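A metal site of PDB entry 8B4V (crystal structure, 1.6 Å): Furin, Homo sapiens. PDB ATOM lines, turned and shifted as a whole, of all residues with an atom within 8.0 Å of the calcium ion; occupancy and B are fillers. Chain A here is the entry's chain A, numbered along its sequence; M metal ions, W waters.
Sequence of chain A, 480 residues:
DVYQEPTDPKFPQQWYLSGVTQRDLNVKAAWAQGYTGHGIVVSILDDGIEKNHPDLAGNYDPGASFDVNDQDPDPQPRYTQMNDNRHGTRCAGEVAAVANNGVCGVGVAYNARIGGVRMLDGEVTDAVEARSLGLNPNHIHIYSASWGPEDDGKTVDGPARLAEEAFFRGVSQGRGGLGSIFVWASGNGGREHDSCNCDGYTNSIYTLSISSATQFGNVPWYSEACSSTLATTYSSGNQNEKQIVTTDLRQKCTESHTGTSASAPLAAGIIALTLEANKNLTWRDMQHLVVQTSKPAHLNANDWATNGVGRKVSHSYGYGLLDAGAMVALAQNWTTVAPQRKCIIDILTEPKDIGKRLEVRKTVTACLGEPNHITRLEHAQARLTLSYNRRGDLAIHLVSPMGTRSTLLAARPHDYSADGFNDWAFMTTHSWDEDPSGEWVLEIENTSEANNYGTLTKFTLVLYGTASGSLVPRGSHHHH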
ATOM      1  N   LYS A  51     -14.590  -2.293  17.517  1.00  0.00           N
ATOM      2  CA  LYS A  51     -14.393  -2.482  16.089  1.00  0.00           C
ATOM      3  C   LYS A  51     -12.911  -2.480  15.720  1.00  0.00           C
ATOM      4  O   LYS A  51     -12.561  -2.990  14.649  1.00  0.00           O
ATOM      5  CB  LYS A  51     -15.132  -1.416  15.283  1.00  0.00           C
ATOM      6  CG  LYS A  51     -14.643   0.003  15.487  1.00  0.00           C
ATOM      7  CD  LYS A  51     -15.616   1.010  14.869  1.00  0.00           C
ATOM      8  CE  LYS A  51     -15.117   2.439  15.070  1.00  0.00           C
ATOM      9  NZ  LYS A  51     -15.129   2.820  16.514  1.00  0.00           N
ATOM     10  N   PHE A  66     -24.436   0.034  14.137  1.00  0.00           N
ATOM     11  CA  PHE A  66     -25.059   1.304  14.495  1.00  0.00           C
ATOM     12  C   PHE A  66     -25.040   1.416  16.015  1.00  0.00           C
ATOM     13  O   PHE A  66     -24.885   0.422  16.731  1.00  0.00           O
ATOM     14  CB  PHE A  66     -26.488   1.423  13.952  1.00  0.00           C
ATOM     15  CG  PHE A  66     -26.935   2.851  13.747  1.00  0.00           C
ATOM     16  CD1 PHE A  66     -26.524   3.559  12.628  1.00  0.00           C
ATOM     17  CD2 PHE A  66     -27.752   3.471  14.672  1.00  0.00           C
ATOM     18  CE1 PHE A  66     -26.918   4.868  12.445  1.00  0.00           C
ATOM     19  CE2 PHE A  66     -28.140   4.796  14.492  1.00  0.00           C
ATOM     20  CZ  PHE A  66     -27.725   5.491  13.373  1.00  0.00           C
ATOM     21  N   ASP A  67     -25.187   2.652  16.500  1.00  0.00           N
ATOM     22  CA  ASP A  67     -25.306   2.919  17.930  1.00  0.00           C
ATOM     23  C   ASP A  67     -26.692   3.510  18.157  1.00  0.00           C
ATOM     24  O   ASP A  67     -26.918   4.708  17.979  1.00  0.00           O
ATOM     25  CB  ASP A  67     -24.202   3.856  18.400  1.00  0.00           C
ATOM     26  CG  ASP A  67     -24.257   4.124  19.895  1.00  0.00           C
ATOM     27  OD1 ASP A  67     -25.291   3.853  20.547  1.00  0.00           O
ATOM     28  OD2 ASP A  67     -23.237   4.654  20.401  1.00  0.00           O
ATOM     29  N   VAL A  68     -27.633   2.645  18.556  1.00  0.00           N
ATOM     30  CA  VAL A  68     -28.989   3.090  18.802  1.00  0.00           C
ATOM     31  C   VAL A  68     -29.081   3.787  20.159  1.00  0.00           C
ATOM     32  O   VAL A  68     -29.949   4.655  20.352  1.00  0.00           O
ATOM     33  CB  VAL A  68     -29.944   1.889  18.691  1.00  0.00           C
ATOM     34  CG1 VAL A  68     -31.344   2.316  19.019  1.00  0.00           C
ATOM     35  CG2 VAL A  68     -29.849   1.288  17.292  1.00  0.00           C
ATOM     36  N   ASN A  69     -28.193   3.464  21.099  1.00  0.00           N
ATOM     37  CA  ASN A  69     -28.274   4.084  22.416  1.00  0.00           C
ATOM     38  C   ASN A  69     -27.938   5.576  22.347  1.00  0.00           C
ATOM     39  O   ASN A  69     -28.602   6.389  23.002  1.00  0.00           O
ATOM     40  CB  ASN A  69     -27.342   3.386  23.405  1.00  0.00           C
ATOM     41  CG  ASN A  69     -27.792   1.973  23.750  1.00  0.00           C
ATOM     42  OD1 ASN A  69     -26.998   1.035  23.728  1.00  0.00           O
ATOM     43  ND2 ASN A  69     -29.070   1.818  24.081  1.00  0.00           N
ATOM     44  N   ASP A  70     -26.916   5.954  21.588  1.00  0.00           N
ATOM     45  CA  ASP A  70     -26.499   7.350  21.477  1.00  0.00           C
ATOM     46  C   ASP A  70     -26.857   7.969  20.136  1.00  0.00           C
ATOM     47  O   ASP A  70     -26.543   9.150  19.913  1.00  0.00           O
ATOM     48  CB  ASP A  70     -24.977   7.475  21.698  1.00  0.00           C
ATOM     49  CG  ASP A  70     -24.599   7.429  23.170  1.00  0.00           C
ATOM     50  OD1 ASP A  70     -25.481   7.559  24.040  1.00  0.00           O
ATOM     51  OD2 ASP A  70     -23.394   7.270  23.445  1.00  0.00           O
ATOM     52  N   GLN A  71     -27.481   7.213  19.238  1.00  0.00           N
ATOM     53  CA  GLN A  71     -27.949   7.687  17.938  1.00  0.00           C
ATOM     54  C   GLN A  71     -26.777   8.227  17.100  1.00  0.00           C
ATOM     55  O   GLN A  71     -26.699   9.415  16.766  1.00  0.00           O
ATOM     56  CB  GLN A  71     -29.068   8.732  18.103  1.00  0.00           C
ATOM     57  CG  GLN A  71     -30.260   8.216  18.922  1.00  0.00           C
ATOM     58  CD  GLN A  71     -31.496   9.102  18.813  1.00  0.00           C
ATOM     59  N   ASP A  72     -25.866   7.328  16.769  1.00  0.00           N
ATOM     60  CA  ASP A  72     -24.746   7.622  15.879  1.00  0.00           C
ATOM     61  C   ASP A  72     -24.308   6.307  15.235  1.00  0.00           C
ATOM     62  O   ASP A  72     -24.807   5.239  15.601  1.00  0.00           O
ATOM     63  CB  ASP A  72     -23.587   8.309  16.628  1.00  0.00           C
ATOM     64  CG  ASP A  72     -22.907   7.408  17.646  1.00  0.00           C
ATOM     65  OD1 ASP A  72     -22.279   6.409  17.232  1.00  0.00           O
ATOM     66  OD2 ASP A  72     -22.961   7.715  18.855  1.00  0.00           O
ATOM     67  N   PRO A  73     -23.419   6.361  14.242  1.00  0.00           N
ATOM     68  CA  PRO A  73     -23.097   5.142  13.487  1.00  0.00           C
ATOM     69  C   PRO A  73     -22.093   4.230  14.168  1.00  0.00           C
ATOM     70  O   PRO A  73     -21.902   3.100  13.699  1.00  0.00           O
ATOM     71  CB  PRO A  73     -22.516   5.668  12.161  1.00  0.00           C
ATOM     72  CG  PRO A  73     -22.809   7.133  12.143  1.00  0.00           C
ATOM     73  CD  PRO A  73     -22.875   7.567  13.581  1.00  0.00           C
ATOM     74  N   ASP A  74     -21.443   4.693  15.235  1.00  0.00           N
ATOM     75  CA  ASP A  74     -20.244   4.079  15.765  1.00  0.00           C
ATOM     76  C   ASP A  74     -20.590   3.255  16.998  1.00  0.00           C
ATOM     77  O   ASP A  74     -20.886   3.837  18.049  1.00  0.00           O
ATOM     78  CB  ASP A  74     -19.221   5.172  16.104  1.00  0.00           C
ATOM     79  CG  ASP A  74     -17.918   4.627  16.659  1.00  0.00           C
ATOM     80  OD1 ASP A  74     -17.791   3.404  16.892  1.00  0.00           O
ATOM     81  OD2 ASP A  74     -17.003   5.438  16.887  1.00  0.00           O
ATOM     82  N   PRO A  75     -20.545   1.918  16.919  1.00  0.00           N
ATOM     83  CA  PRO A  75     -20.998   1.075  18.035  1.00  0.00           C
ATOM     84  C   PRO A  75     -19.939   0.788  19.086  1.00  0.00           C
ATOM     85  O   PRO A  75     -20.083  -0.150  19.875  1.00  0.00           O
ATOM     86  CB  PRO A  75     -21.399  -0.224  17.325  1.00  0.00           C
ATOM     87  CG  PRO A  75     -20.295  -0.319  16.255  1.00  0.00           C
ATOM     88  CD  PRO A  75     -20.140   1.094  15.756  1.00  0.00           C
ATOM     89  N   GLN A  76     -18.870   1.566  19.107  1.00  0.00           N
ATOM     90  CA  GLN A  76     -17.806   1.302  20.064  1.00  0.00           C
ATOM     91  C   GLN A  76     -18.374   1.216  21.476  1.00  0.00           C
ATOM     92  O   GLN A  76     -19.227   2.042  21.849  1.00  0.00           O
ATOM     93  CB  GLN A  76     -16.737   2.401  19.979  1.00  0.00           C
ATOM     94  CG  GLN A  76     -15.438   2.059  20.684  1.00  0.00           C
ATOM     95  CD  GLN A  76     -14.533   1.147  19.874  1.00  0.00           C
ATOM     96  OE1 GLN A  76     -14.683   1.001  18.666  1.00  0.00           O
ATOM     97  NE2 GLN A  76     -13.557   0.527  20.549  1.00  0.00           N
ATOM     98  N   PRO A  77     -17.923   0.259  22.283  1.00  0.00           N
ATOM     99  CA  PRO A  77     -18.458   0.153  23.644  1.00  0.00           C
ATOM    100  C   PRO A  77     -18.040   1.323  24.527  1.00  0.00           C
ATOM    101  O   PRO A  77     -17.025   1.988  24.312  1.00  0.00           O
ATOM    102  CB  PRO A  77     -17.859  -1.159  24.183  1.00  0.00           C
ATOM    103  CG  PRO A  77     -17.385  -1.892  22.975  1.00  0.00           C
ATOM    104  CD  PRO A  77     -17.014  -0.852  21.955  1.00  0.00           C
ATOM    105  N   ARG A  78     -18.862   1.555  25.558  1.00  0.00           N
ATOM    106  CA  ARG A  78     -18.539   2.482  26.643  1.00  0.00           C
ATOM    107  C   ARG A  78     -17.637   1.783  27.659  1.00  0.00           C
ATOM    108  O   ARG A  78     -18.033   0.776  28.250  1.00  0.00           O
ATOM    109  CB  ARG A  78     -19.828   2.986  27.288  1.00  0.00           C
ATOM    110  CG  ARG A  78     -19.659   3.939  28.452  1.00  0.00           C
ATOM    111  CD  ARG A  78     -21.017   4.470  28.928  1.00  0.00           C
ATOM    112  NE  ARG A  78     -21.828   3.353  29.385  1.00  0.00           N
ATOM    113  CZ  ARG A  78     -21.861   2.906  30.639  1.00  0.00           C
ATOM    114  NH1 ARG A  78     -22.617   1.854  30.947  1.00  0.00           N
ATOM    115  NH2 ARG A  78     -21.137   3.497  31.584  1.00  0.00           N
ATOM    116  N   ARG A 118     -25.008  -1.220  19.089  1.00  0.00           N
ATOM    117  CA  ARG A 118     -24.943  -0.827  20.492  1.00  0.00           C
ATOM    118  C   ARG A 118     -26.361  -0.398  20.866  1.00  0.00           C
ATOM    119  O   ARG A 118     -26.816   0.679  20.493  1.00  0.00           O
ATOM    120  CB  ARG A 118     -23.922   0.281  20.698  1.00  0.00           C
ATOM    121  CG  ARG A 118     -23.788   0.750  22.129  1.00  0.00           C
ATOM    122  CD  ARG A 118     -22.618   1.742  22.335  1.00  0.00           C
ATOM    123  NE  ARG A 118     -22.598   2.197  23.729  1.00  0.00           N
ATOM    124  CZ  ARG A 118     -22.986   3.410  24.142  1.00  0.00           C
ATOM    125  NH1 ARG A 118     -22.964   3.691  25.432  1.00  0.00           N
ATOM    126  NH2 ARG A 118     -23.383   4.329  23.268  1.00  0.00           N
HETATM  127 CA    CA M   1     -21.396   5.756  19.482  1.00  0.00          CA
HETATM  128  O   HOH W   1     -21.353   7.080  21.577  1.00  0.00           O
HETATM  129  O   HOH W   2     -19.492   7.089  19.036  1.00  0.00           O
HETATM  130  O   HOH W   3     -19.794   4.560  20.814  1.00  0.00           O
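Within 4 Å of the calcium ion: Asp 67, Asp 72 and Asp 74.
The nearest printed residue that does not touch the calcium ion is Arg 118 (4.5 Å).
N of Asp 70 is in hydrogen-bond range of OD1 of Asp 67.
The backbone NH (N) of Gln 76 sits at hydrogen-bond distance from the side-chain carboxylate (OD1) of Asp 74 (3.1 Å).
OD1 of Asp 67 lies within salt-bridge range of NH2 of Arg 118, 3.4 Å away.
The side-chain carboxylate (OD1) of Asp 67 is in hydrogen-bond range of the backbone NH (N) of Asn 69 (3.0 Å).
The side-chain amino group of Lys 51 is in salt-bridge range of the side-chain carboxylate of Asp 74.
The calcium ion is bound by the side-chain carboxylate (OD2) of Asp 67 (2.3 Å).
Water W2 binds the calcium ion, 2.4 Å away.
The calcium ion is bound by water W3 (2.4 Å).
O of Asp 74 is bound to the calcium ion (2.4 Å).
The calcium ion is bound by water W1 (2.5 Å).
OD1 of Asp 72 is bound to the calcium ion.
The side-chain carboxylate (OD2) of Asp 72 binds the calcium ion, at 2.6 Å.
The calcium ion has seven donor atoms within binding distance.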
